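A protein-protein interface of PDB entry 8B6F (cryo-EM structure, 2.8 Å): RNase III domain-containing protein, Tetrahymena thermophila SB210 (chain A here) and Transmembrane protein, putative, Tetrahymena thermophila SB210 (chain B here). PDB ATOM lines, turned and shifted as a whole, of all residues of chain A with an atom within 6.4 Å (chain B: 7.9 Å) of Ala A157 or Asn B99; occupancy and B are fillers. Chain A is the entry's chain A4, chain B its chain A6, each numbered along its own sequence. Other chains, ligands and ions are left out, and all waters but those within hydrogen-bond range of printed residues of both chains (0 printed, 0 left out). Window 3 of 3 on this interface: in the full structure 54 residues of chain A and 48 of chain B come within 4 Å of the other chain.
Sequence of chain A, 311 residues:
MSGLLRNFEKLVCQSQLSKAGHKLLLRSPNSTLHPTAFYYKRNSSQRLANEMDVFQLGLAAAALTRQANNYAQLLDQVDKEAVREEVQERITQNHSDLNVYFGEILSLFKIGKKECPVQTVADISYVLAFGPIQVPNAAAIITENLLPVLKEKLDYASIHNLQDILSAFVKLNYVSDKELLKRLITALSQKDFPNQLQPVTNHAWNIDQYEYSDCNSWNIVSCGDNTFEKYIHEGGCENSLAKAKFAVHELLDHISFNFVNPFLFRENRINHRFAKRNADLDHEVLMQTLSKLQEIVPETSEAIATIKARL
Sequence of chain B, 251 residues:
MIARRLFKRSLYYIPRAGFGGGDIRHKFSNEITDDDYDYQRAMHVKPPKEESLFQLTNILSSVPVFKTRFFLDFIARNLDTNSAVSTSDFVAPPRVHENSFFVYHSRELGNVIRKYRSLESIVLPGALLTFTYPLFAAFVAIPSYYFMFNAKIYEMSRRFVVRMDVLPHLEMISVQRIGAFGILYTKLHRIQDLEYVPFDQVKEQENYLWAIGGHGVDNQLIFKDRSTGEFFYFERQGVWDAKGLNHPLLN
A ring nitrogen (ND1) of His B97 sits close to the backbone NH (N) of Asn B99 (3.2 Å). The side-chain hydroxyl (OG) of Ser B100 is in hydrogen-bond range of the backbone NH (N) of His B97, 2.9 Å away. The side-chain amide nitrogen (ND2) of Asn B99 is in hydrogen-bond range of a ring nitrogen (ND1) of His B169. The backbone carbonyl oxygen (O) of Ala A157 sits close to the side-chain amino group (NZ) of Lys A191 (3.2 Å).
OE2 of Glu B171 touches CE of Lys A153, at 3.4 Å. CD1 of Tyr A156 touches CB of Pro B168, 3.7 Å away. CE1 of Tyr A156 touches NE2 of His B247, at 3.7 Å. O of Ala A157 touches ND2 of Asn B99, 3.6 Å away. CE1 of His B97 touches OG of Ser A158, at 3.9 Å. CA of Ser A158 touches ND2 of Asn B99, at 3.7 Å. Ser A158 touches His B169. CB of His B169 touches ND2 of Asn A161, at 3.3 Å.
Printed residues of chain A that touch a printed residue of chain B: Val A118, Lys A153, Tyr A156, Ala A157, Ser A158, Ile A159, Asn A161 and Lys A191. Hydrophobic or aromatic side chains of chain A within 4 Å of the printed part of chain B: Tyr A156 and Ile A159. Hydrophobic or aromatic side chains of chain B within 4 Å of the printed part of chain A: His B97, Pro B168, His B169 and His B247. Along chain B the printed residues that touch a printed residue of chain A span positions 97 to 247. Among the printed residues, 14 pairs touch across the chains. Among the printed residues, no Asp or Glu carboxylate lies within 4 Å of a Lys or Arg side-chain nitrogen of the other chain.
Of the printed residues of chain A, Glu B98 touches Ser A158 and Ile A159. Printed residues of chain B within 4 Å of Val A118: His B169 (3.4 Å). Of the printed residues of chain B, Ser A158 touches His B97, Glu B98, Asn B99 and His B169. Of the printed residues of chain A, His B247 touches Tyr A156 (3.7 Å). The nearest residue of chain B that does not touch Ala A157 is His B169 (4.5 Å). The nearest residue of chain A that does not touch Asn B99 is Asp A155 (4.9 Å).
NZ of Lys A191 is in hydrogen-bond range of OD1 of Asn B99, 2.8 Å away. The backbone NH (N) of Ile A159 sits at hydrogen-bond distance from the side-chain carboxylate (OE2) of Glu B98, 3.4 Å away. The backbone carbonyl oxygen (O) of Tyr A156 sits close to the backbone NH (N) of His B169 (3.4 Å). O of Tyr A156 lies within hydrogen-bond range of ND2 of Asn B99 (2.8 Å). OE2 of Glu B98 is in hydrogen-bond range of OG of Ser A158, at 2.5 Å. The backbone NH (N) of Val A118 is in hydrogen-bond range of the backbone carbonyl oxygen (O) of His B169, at 3.4 Å.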
ATOM      1  N   VAL A 118      -8.021 -22.229 -17.720  1.00  0.00           N
ATOM      2  CA  VAL A 118      -8.993 -22.117 -16.636  1.00  0.00           C
ATOM      3  C   VAL A 118      -8.480 -21.185 -15.547  1.00  0.00           C
ATOM      4  O   VAL A 118      -9.252 -20.424 -14.950  1.00  0.00           O
ATOM      5  CB  VAL A 118      -9.322 -23.508 -16.066  1.00  0.00           C
ATOM      6  CG1 VAL A 118     -10.418 -23.404 -15.017  1.00  0.00           C
ATOM      7  CG2 VAL A 118      -9.732 -24.458 -17.172  1.00  0.00           C
ATOM      8  N   LEU A 150     -15.016 -21.209 -19.128  1.00  0.00           N
ATOM      9  CA  LEU A 150     -15.213 -22.056 -17.956  1.00  0.00           C
ATOM     10  C   LEU A 150     -16.037 -23.288 -18.299  1.00  0.00           C
ATOM     11  O   LEU A 150     -15.704 -24.403 -17.881  1.00  0.00           O
ATOM     12  CB  LEU A 150     -15.885 -21.253 -16.843  1.00  0.00           C
ATOM     13  CG  LEU A 150     -16.240 -22.025 -15.571  1.00  0.00           C
ATOM     14  CD1 LEU A 150     -14.995 -22.626 -14.942  1.00  0.00           C
ATOM     15  CD2 LEU A 150     -16.959 -21.121 -14.587  1.00  0.00           C
ATOM     16  N   LYS A 153     -13.759 -25.734 -20.388  1.00  0.00           N
ATOM     17  CA  LYS A 153     -12.562 -26.286 -19.763  1.00  0.00           C
ATOM     18  C   LYS A 153     -12.735 -26.527 -18.266  1.00  0.00           C
ATOM     19  O   LYS A 153     -11.754 -26.537 -17.521  1.00  0.00           O
ATOM     20  CB  LYS A 153     -11.368 -25.364 -20.005  1.00  0.00           C
ATOM     21  CG  LYS A 153     -11.035 -25.143 -21.470  1.00  0.00           C
ATOM     22  CD  LYS A 153      -9.798 -24.272 -21.621  1.00  0.00           C
ATOM     23  CE  LYS A 153      -9.435 -24.061 -23.081  1.00  0.00           C
ATOM     24  NZ  LYS A 153     -10.499 -23.334 -23.825  1.00  0.00           N
ATOM     25  N   LEU A 154     -13.972 -26.729 -17.807  1.00  0.00           N
ATOM     26  CA  LEU A 154     -14.181 -26.977 -16.385  1.00  0.00           C
ATOM     27  C   LEU A 154     -13.442 -28.224 -15.920  1.00  0.00           C
ATOM     28  O   LEU A 154     -12.980 -28.281 -14.776  1.00  0.00           O
ATOM     29  CB  LEU A 154     -15.676 -27.100 -16.088  1.00  0.00           C
ATOM     30  CG  LEU A 154     -16.087 -26.978 -14.617  1.00  0.00           C
ATOM     31  CD1 LEU A 154     -17.474 -26.373 -14.523  1.00  0.00           C
ATOM     32  CD2 LEU A 154     -16.052 -28.321 -13.908  1.00  0.00           C
ATOM     33  N   ASP A 155     -13.307 -29.226 -16.792  1.00  0.00           N
ATOM     34  CA  ASP A 155     -12.618 -30.453 -16.407  1.00  0.00           C
ATOM     35  C   ASP A 155     -11.161 -30.180 -16.054  1.00  0.00           C
ATOM     36  O   ASP A 155     -10.620 -30.774 -15.113  1.00  0.00           O
ATOM     37  CB  ASP A 155     -12.711 -31.481 -17.534  1.00  0.00           C
ATOM     38  CG  ASP A 155     -14.137 -31.917 -17.808  1.00  0.00           C
ATOM     39  OD1 ASP A 155     -15.048 -31.465 -17.083  1.00  0.00           O
ATOM     40  OD2 ASP A 155     -14.347 -32.710 -18.749  1.00  0.00           O
ATOM     41  N   TYR A 156     -10.508 -29.289 -16.798  1.00  0.00           N
ATOM     42  CA  TYR A 156      -9.122 -28.941 -16.519  1.00  0.00           C
ATOM     43  C   TYR A 156      -8.963 -28.134 -15.238  1.00  0.00           C
ATOM     44  O   TYR A 156      -7.828 -27.932 -14.796  1.00  0.00           O
ATOM     45  CB  TYR A 156      -8.535 -28.148 -17.689  1.00  0.00           C
ATOM     46  CG  TYR A 156      -8.511 -28.890 -19.007  1.00  0.00           C
ATOM     47  CD1 TYR A 156      -8.444 -30.276 -19.051  1.00  0.00           C
ATOM     48  CD2 TYR A 156      -8.554 -28.197 -20.210  1.00  0.00           C
ATOM     49  CE1 TYR A 156      -8.420 -30.953 -20.255  1.00  0.00           C
ATOM     50  CE2 TYR A 156      -8.530 -28.863 -21.418  1.00  0.00           C
ATOM     51  CZ  TYR A 156      -8.463 -30.241 -21.434  1.00  0.00           C
ATOM     52  OH  TYR A 156      -8.441 -30.906 -22.637  1.00  0.00           O
ATOM     53  N   ALA A 157     -10.057 -27.675 -14.638  1.00  0.00           N
ATOM     54  CA  ALA A 157      -9.961 -26.808 -13.472  1.00  0.00           C
ATOM     55  C   ALA A 157      -9.245 -27.513 -12.326  1.00  0.00           C
ATOM     56  O   ALA A 157      -9.413 -28.716 -12.110  1.00  0.00           O
ATOM     57  CB  ALA A 157     -11.356 -26.375 -13.024  1.00  0.00           C
ATOM     58  N   SER A 158      -8.440 -26.751 -11.594  1.00  0.00           N
ATOM     59  CA  SER A 158      -7.748 -27.243 -10.416  1.00  0.00           C
ATOM     60  C   SER A 158      -8.577 -26.971  -9.162  1.00  0.00           C
ATOM     61  O   SER A 158      -9.612 -26.306  -9.200  1.00  0.00           O
ATOM     62  CB  SER A 158      -6.373 -26.588 -10.298  1.00  0.00           C
ATOM     63  OG  SER A 158      -5.728 -26.965  -9.095  1.00  0.00           O
ATOM     64  N   ILE A 159      -8.104 -27.499  -8.031  1.00  0.00           N
ATOM     65  CA  ILE A 159      -8.803 -27.284  -6.767  1.00  0.00           C
ATOM     66  C   ILE A 159      -8.810 -25.803  -6.419  1.00  0.00           C
ATOM     67  O   ILE A 159      -9.844 -25.236  -6.051  1.00  0.00           O
ATOM     68  CB  ILE A 159      -8.168 -28.124  -5.645  1.00  0.00           C
ATOM     69  CG1 ILE A 159      -8.255 -29.610  -5.988  1.00  0.00           C
ATOM     70  CG2 ILE A 159      -8.858 -27.848  -4.316  1.00  0.00           C
ATOM     71  CD1 ILE A 159      -7.476 -30.499  -5.056  1.00  0.00           C
ATOM     72  N   ASN A 161      -8.445 -23.267  -8.458  1.00  0.00           N
ATOM     73  CA  ASN A 161      -9.263 -22.538  -9.419  1.00  0.00           C
ATOM     74  C   ASN A 161     -10.747 -22.708  -9.121  1.00  0.00           C
ATOM     75  O   ASN A 161     -11.514 -21.741  -9.188  1.00  0.00           O
ATOM     76  CB  ASN A 161      -8.943 -23.007 -10.836  1.00  0.00           C
ATOM     77  CG  ASN A 161      -7.498 -22.763 -11.211  1.00  0.00           C
ATOM     78  OD1 ASN A 161      -6.862 -21.838 -10.709  1.00  0.00           O
ATOM     79  ND2 ASN A 161      -6.971 -23.596 -12.096  1.00  0.00           N
ATOM     80  N   LEU A 162     -11.172 -23.929  -8.791  1.00  0.00           N
ATOM     81  CA  LEU A 162     -12.575 -24.141  -8.450  1.00  0.00           C
ATOM     82  C   LEU A 162     -12.962 -23.350  -7.208  1.00  0.00           C
ATOM     83  O   LEU A 162     -14.025 -22.721  -7.170  1.00  0.00           O
ATOM     84  CB  LEU A 162     -12.848 -25.631  -8.243  1.00  0.00           C
ATOM     85  CG  LEU A 162     -12.826 -26.507  -9.499  1.00  0.00           C
ATOM     86  CD1 LEU A 162     -12.950 -27.972  -9.127  1.00  0.00           C
ATOM     87  CD2 LEU A 162     -13.933 -26.112 -10.467  1.00  0.00           C
ATOM     88  N   ILE A 165     -13.187 -19.662  -8.138  1.00  0.00           N
ATOM     89  CA  ILE A 165     -14.351 -19.375  -8.973  1.00  0.00           C
ATOM     90  C   ILE A 165     -15.616 -19.366  -8.128  1.00  0.00           C
ATOM     91  O   ILE A 165     -16.466 -18.476  -8.257  1.00  0.00           O
ATOM     92  CB  ILE A 165     -14.441 -20.391 -10.126  1.00  0.00           C
ATOM     93  CG1 ILE A 165     -13.306 -20.147 -11.123  1.00  0.00           C
ATOM     94  CG2 ILE A 165     -15.789 -20.297 -10.830  1.00  0.00           C
ATOM     95  CD1 ILE A 165     -13.104 -21.272 -12.107  1.00  0.00           C
ATOM     96  N   LEU A 184     -19.662 -27.158 -10.850  1.00  0.00           N
ATOM     97  CA  LEU A 184     -18.448 -26.787 -10.131  1.00  0.00           C
ATOM     98  C   LEU A 184     -18.370 -27.491  -8.781  1.00  0.00           C
ATOM     99  O   LEU A 184     -17.302 -27.968  -8.381  1.00  0.00           O
ATOM    100  CB  LEU A 184     -18.394 -25.273  -9.945  1.00  0.00           C
ATOM    101  CG  LEU A 184     -18.201 -24.449 -11.217  1.00  0.00           C
ATOM    102  CD1 LEU A 184     -18.519 -22.989 -10.954  1.00  0.00           C
ATOM    103  CD2 LEU A 184     -16.776 -24.592 -11.723  1.00  0.00           C
ATOM    104  N   ALA A 187     -17.512 -31.167  -9.276  1.00  0.00           N
ATOM    105  CA  ALA A 187     -16.119 -31.297  -9.685  1.00  0.00           C
ATOM    106  C   ALA A 187     -15.182 -31.113  -8.498  1.00  0.00           C
ATOM    107  O   ALA A 187     -14.215 -31.867  -8.338  1.00  0.00           O
ATOM    108  CB  ALA A 187     -15.797 -30.285 -10.783  1.00  0.00           C
ATOM    109  N   LYS A 191     -12.581 -33.890  -6.882  1.00  0.00           N
ATOM    110  CA  LYS A 191     -11.149 -33.638  -6.799  1.00  0.00           C
ATOM    111  C   LYS A 191     -10.555 -34.288  -5.553  1.00  0.00           C
ATOM    112  O   LYS A 191     -11.256 -34.627  -4.597  1.00  0.00           O
ATOM    113  CB  LYS A 191     -10.867 -32.135  -6.786  1.00  0.00           C
ATOM    114  CG  LYS A 191     -10.864 -31.483  -8.162  1.00  0.00           C
ATOM    115  CD  LYS A 191      -9.650 -31.912  -8.979  1.00  0.00           C
ATOM    116  CE  LYS A 191      -9.592 -31.176 -10.309  1.00  0.00           C
ATOM    117  NZ  LYS A 191      -8.423 -31.597 -11.129  1.00  0.00           N
ATOM    118  N   ARG B  95       2.498 -37.967  -9.128  1.00  0.00           N
ATOM    119  CA  ARG B  95       2.163 -36.722  -9.804  1.00  0.00           C
ATOM    120  C   ARG B  95       2.915 -35.554  -9.178  1.00  0.00           C
ATOM    121  O   ARG B  95       3.034 -35.452  -7.955  1.00  0.00           O
ATOM    122  CB  ARG B  95       0.656 -36.470  -9.745  1.00  0.00           C
ATOM    123  CG  ARG B  95       0.078 -36.446  -8.337  1.00  0.00           C
ATOM    124  CD  ARG B  95      -1.384 -36.024  -8.347  1.00  0.00           C
ATOM    125  NE  ARG B  95      -2.242 -36.998  -9.011  1.00  0.00           N
ATOM    126  CZ  ARG B  95      -2.897 -37.973  -8.396  1.00  0.00           C
ATOM    127  NH1 ARG B  95      -2.811 -38.149  -7.088  1.00  0.00           N
ATOM    128  NH2 ARG B  95      -3.662 -38.793  -9.111  1.00  0.00           N
ATOM    129  N   VAL B  96       3.437 -34.672 -10.033  1.00  0.00           N
ATOM    130  CA  VAL B  96       4.124 -33.480  -9.545  1.00  0.00           C
ATOM    131  C   VAL B  96       3.128 -32.504  -8.931  1.00  0.00           C
ATOM    132  O   VAL B  96       3.413 -31.864  -7.911  1.00  0.00           O
ATOM    133  CB  VAL B  96       4.928 -32.831 -10.686  1.00  0.00           C
ATOM    134  CG1 VAL B  96       5.516 -31.500 -10.247  1.00  0.00           C
ATOM    135  CG2 VAL B  96       6.033 -33.764 -11.149  1.00  0.00           C
ATOM    136  N   HIS B  97       1.954 -32.370  -9.540  1.00  0.00           N
ATOM    137  CA  HIS B  97       0.909 -31.482  -9.061  1.00  0.00           C
ATOM    138  C   HIS B  97      -0.400 -32.252  -8.994  1.00  0.00           C
ATOM    139  O   HIS B  97      -0.629 -33.185  -9.767  1.00  0.00           O
ATOM    140  CB  HIS B  97       0.755 -30.257  -9.973  1.00  0.00           C
ATOM    141  CG  HIS B  97      -0.126 -29.187  -9.408  1.00  0.00           C
ATOM    142  ND1 HIS B  97      -1.454 -29.057  -9.753  1.00  0.00           N
ATOM    143  CD2 HIS B  97       0.132 -28.193  -8.526  1.00  0.00           C
ATOM    144  CE1 HIS B  97      -1.976 -28.031  -9.106  1.00  0.00           C
ATOM    145  NE2 HIS B  97      -1.035 -27.489  -8.354  1.00  0.00           N
ATOM    146  N   GLU B  98      -1.267 -31.845  -8.066  1.00  0.00           N
ATOM    147  CA  GLU B  98      -2.499 -32.585  -7.826  1.00  0.00           C
ATOM    148  C   GLU B  98      -3.377 -32.669  -9.067  1.00  0.00           C
ATOM    149  O   GLU B  98      -4.229 -33.559  -9.147  1.00  0.00           O
ATOM    150  CB  GLU B  98      -3.277 -31.952  -6.668  1.00  0.00           C
ATOM    151  CG  GLU B  98      -3.645 -30.485  -6.864  1.00  0.00           C
ATOM    152  CD  GLU B  98      -4.896 -30.290  -7.699  1.00  0.00           C
ATOM    153  OE1 GLU B  98      -5.636 -31.273  -7.914  1.00  0.00           O
ATOM    154  OE2 GLU B  98      -5.143 -29.147  -8.137  1.00  0.00           O
ATOM    155  N   ASN B  99      -3.194 -31.769 -10.033  1.00  0.00           N
ATOM    156  CA  ASN B  99      -4.004 -31.750 -11.242  1.00  0.00           C
ATOM    157  C   ASN B  99      -3.219 -32.106 -12.499  1.00  0.00           C
ATOM    158  O   ASN B  99      -3.813 -32.188 -13.578  1.00  0.00           O
ATOM    159  CB  ASN B  99      -4.646 -30.367 -11.413  1.00  0.00           C
ATOM    160  CG  ASN B  99      -5.708 -30.346 -12.495  1.00  0.00           C
ATOM    161  OD1 ASN B  99      -6.266 -31.381 -12.853  1.00  0.00           O
ATOM    162  ND2 ASN B  99      -5.990 -29.162 -13.021  1.00  0.00           N
ATOM    163  N   SER B 100      -1.914 -32.327 -12.393  1.00  0.00           N
ATOM    164  CA  SER B 100      -1.083 -32.597 -13.556  1.00  0.00           C
ATOM    165  C   SER B 100      -1.071 -34.086 -13.883  1.00  0.00           C
ATOM    166  O   SER B 100      -1.441 -34.932 -13.067  1.00  0.00           O
ATOM    167  CB  SER B 100       0.346 -32.105 -13.322  1.00  0.00           C
ATOM    168  OG  SER B 100       0.975 -32.832 -12.280  1.00  0.00           O
ATOM    169  N   PHE B 101      -0.640 -34.400 -15.106  1.00  0.00           N
ATOM    170  CA  PHE B 101      -0.443 -35.774 -15.546  1.00  0.00           C
ATOM    171  C   PHE B 101       0.898 -35.894 -16.255  1.00  0.00           C
ATOM    172  O   PHE B 101       1.276 -35.018 -17.037  1.00  0.00           O
ATOM    173  CB  PHE B 101      -1.576 -36.240 -16.471  1.00  0.00           C
ATOM    174  CG  PHE B 101      -1.778 -35.367 -17.676  1.00  0.00           C
ATOM    175  CD1 PHE B 101      -1.036 -35.567 -18.828  1.00  0.00           C
ATOM    176  CD2 PHE B 101      -2.732 -34.363 -17.664  1.00  0.00           C
ATOM    177  CE1 PHE B 101      -1.229 -34.772 -19.939  1.00  0.00           C
ATOM    178  CE2 PHE B 101      -2.929 -33.564 -18.772  1.00  0.00           C
ATOM    179  CZ  PHE B 101      -2.178 -33.769 -19.911  1.00  0.00           C
ATOM    180  N   PHE B 102       1.613 -36.979 -15.975  1.00  0.00           N
ATOM    181  CA  PHE B 102       2.959 -37.162 -16.500  1.00  0.00           C
ATOM    182  C   PHE B 102       2.917 -37.661 -17.940  1.00  0.00           C
ATOM    183  O   PHE B 102       1.955 -38.305 -18.368  1.00  0.00           O
ATOM    184  CB  PHE B 102       3.743 -38.140 -15.623  1.00  0.00           C
ATOM    185  CG  PHE B 102       4.132 -39.410 -16.320  1.00  0.00           C
ATOM    186  CD1 PHE B 102       3.246 -40.469 -16.409  1.00  0.00           C
ATOM    187  CD2 PHE B 102       5.397 -39.552 -16.868  1.00  0.00           C
ATOM    188  CE1 PHE B 102       3.608 -41.640 -17.045  1.00  0.00           C
ATOM    189  CE2 PHE B 102       5.765 -40.719 -17.504  1.00  0.00           C
ATOM    190  CZ  PHE B 102       4.870 -41.765 -17.593  1.00  0.00           C
ATOM    191  N   VAL B 166       2.322 -32.383 -17.472  1.00  0.00           N
ATOM    192  CA  VAL B 166       1.473 -31.339 -18.031  1.00  0.00           C
ATOM    193  C   VAL B 166       0.457 -30.922 -16.979  1.00  0.00           C
ATOM    194  O   VAL B 166      -0.234 -31.769 -16.402  1.00  0.00           O
ATOM    195  CB  VAL B 166       0.765 -31.809 -19.315  1.00  0.00           C
ATOM    196  CG1 VAL B 166      -0.145 -30.715 -19.862  1.00  0.00           C
ATOM    197  CG2 VAL B 166       1.784 -32.225 -20.358  1.00  0.00           C
ATOM    198  N   LEU B 167       0.375 -29.617 -16.735  1.00  0.00           N
ATOM    199  CA  LEU B 167      -0.660 -29.040 -15.893  1.00  0.00           C
ATOM    200  C   LEU B 167      -1.748 -28.485 -16.798  1.00  0.00           C
ATOM    201  O   LEU B 167      -1.496 -27.509 -17.521  1.00  0.00           O
ATOM    202  CB  LEU B 167      -0.086 -27.936 -15.008  1.00  0.00           C
ATOM    203  CG  LEU B 167       0.772 -28.371 -13.813  1.00  0.00           C
ATOM    204  CD1 LEU B 167       2.000 -29.159 -14.242  1.00  0.00           C
ATOM    205  CD2 LEU B 167       1.188 -27.161 -12.998  1.00  0.00           C
ATOM    206  N   PRO B 168      -2.960 -29.050 -16.798  1.00  0.00           N
ATOM    207  CA  PRO B 168      -3.973 -28.608 -17.766  1.00  0.00           C
ATOM    208  C   PRO B 168      -4.602 -27.272 -17.414  1.00  0.00           C
ATOM    209  O   PRO B 168      -4.924 -26.487 -18.310  1.00  0.00           O
ATOM    210  CB  PRO B 168      -5.006 -29.742 -17.724  1.00  0.00           C
ATOM    211  CG  PRO B 168      -4.896 -30.285 -16.353  1.00  0.00           C
ATOM    212  CD  PRO B 168      -3.449 -30.161 -15.962  1.00  0.00           C
ATOM    213  N   HIS B 169      -4.789 -26.996 -16.124  1.00  0.00           N
ATOM    214  CA  HIS B 169      -5.402 -25.729 -15.740  1.00  0.00           C
ATOM    215  C   HIS B 169      -4.553 -24.551 -16.199  1.00  0.00           C
ATOM    216  O   HIS B 169      -5.084 -23.543 -16.678  1.00  0.00           O
ATOM    217  CB  HIS B 169      -5.630 -25.682 -14.227  1.00  0.00           C
ATOM    218  CG  HIS B 169      -4.380 -25.816 -13.415  1.00  0.00           C
ATOM    219  ND1 HIS B 169      -3.693 -27.006 -13.293  1.00  0.00           N
ATOM    220  CD2 HIS B 169      -3.704 -24.915 -12.665  1.00  0.00           C
ATOM    221  CE1 HIS B 169      -2.642 -26.827 -12.514  1.00  0.00           C
ATOM    222  NE2 HIS B 169      -2.626 -25.568 -12.117  1.00  0.00           N
ATOM    223  N   LEU B 170      -3.231 -24.656 -16.064  1.00  0.00           N
ATOM    224  CA  LEU B 170      -2.328 -23.657 -16.620  1.00  0.00           C
ATOM    225  C   LEU B 170      -2.061 -23.850 -18.106  1.00  0.00           C
ATOM    226  O   LEU B 170      -1.546 -22.929 -18.748  1.00  0.00           O
ATOM    227  CB  LEU B 170      -0.992 -23.693 -15.877  1.00  0.00           C
ATOM    228  CG  LEU B 170      -0.978 -23.164 -14.447  1.00  0.00           C
ATOM    229  CD1 LEU B 170       0.333 -23.510 -13.766  1.00  0.00           C
ATOM    230  CD2 LEU B 170      -1.214 -21.666 -14.443  1.00  0.00           C
ATOM    231  N   GLU B 171      -2.402 -25.009 -18.665  1.00  0.00           N
ATOM    232  CA  GLU B 171      -2.000 -25.363 -20.023  1.00  0.00           C
ATOM    233  C   GLU B 171      -0.490 -25.227 -20.189  1.00  0.00           C
ATOM    234  O   GLU B 171       0.004 -24.693 -21.184  1.00  0.00           O
ATOM    235  CB  GLU B 171      -2.742 -24.513 -21.056  1.00  0.00           C
ATOM    236  CG  GLU B 171      -4.232 -24.799 -21.126  1.00  0.00           C
ATOM    237  CD  GLU B 171      -4.924 -24.019 -22.226  1.00  0.00           C
ATOM    238  OE1 GLU B 171      -4.229 -23.298 -22.972  1.00  0.00           O
ATOM    239  OE2 GLU B 171      -6.162 -24.126 -22.343  1.00  0.00           O
ATOM    240  N   HIS B 247      -3.320 -36.899 -25.095  1.00  0.00           N
ATOM    241  CA  HIS B 247      -4.151 -35.875 -24.482  1.00  0.00           C
ATOM    242  C   HIS B 247      -4.354 -34.722 -25.464  1.00  0.00           C
ATOM    243  O   HIS B 247      -3.407 -34.316 -26.146  1.00  0.00           O
ATOM    244  CB  HIS B 247      -3.504 -35.361 -23.195  1.00  0.00           C
ATOM    245  CG  HIS B 247      -4.447 -34.615 -22.304  1.00  0.00           C
ATOM    246  ND1 HIS B 247      -5.363 -35.250 -21.492  1.00  0.00           N
ATOM    247  CD2 HIS B 247      -4.624 -33.288 -22.104  1.00  0.00           C
ATOM    248  CE1 HIS B 247      -6.058 -34.346 -20.827  1.00  0.00           C
ATOM    249  NE2 HIS B 247      -5.630 -33.148 -21.180  1.00  0.00           N
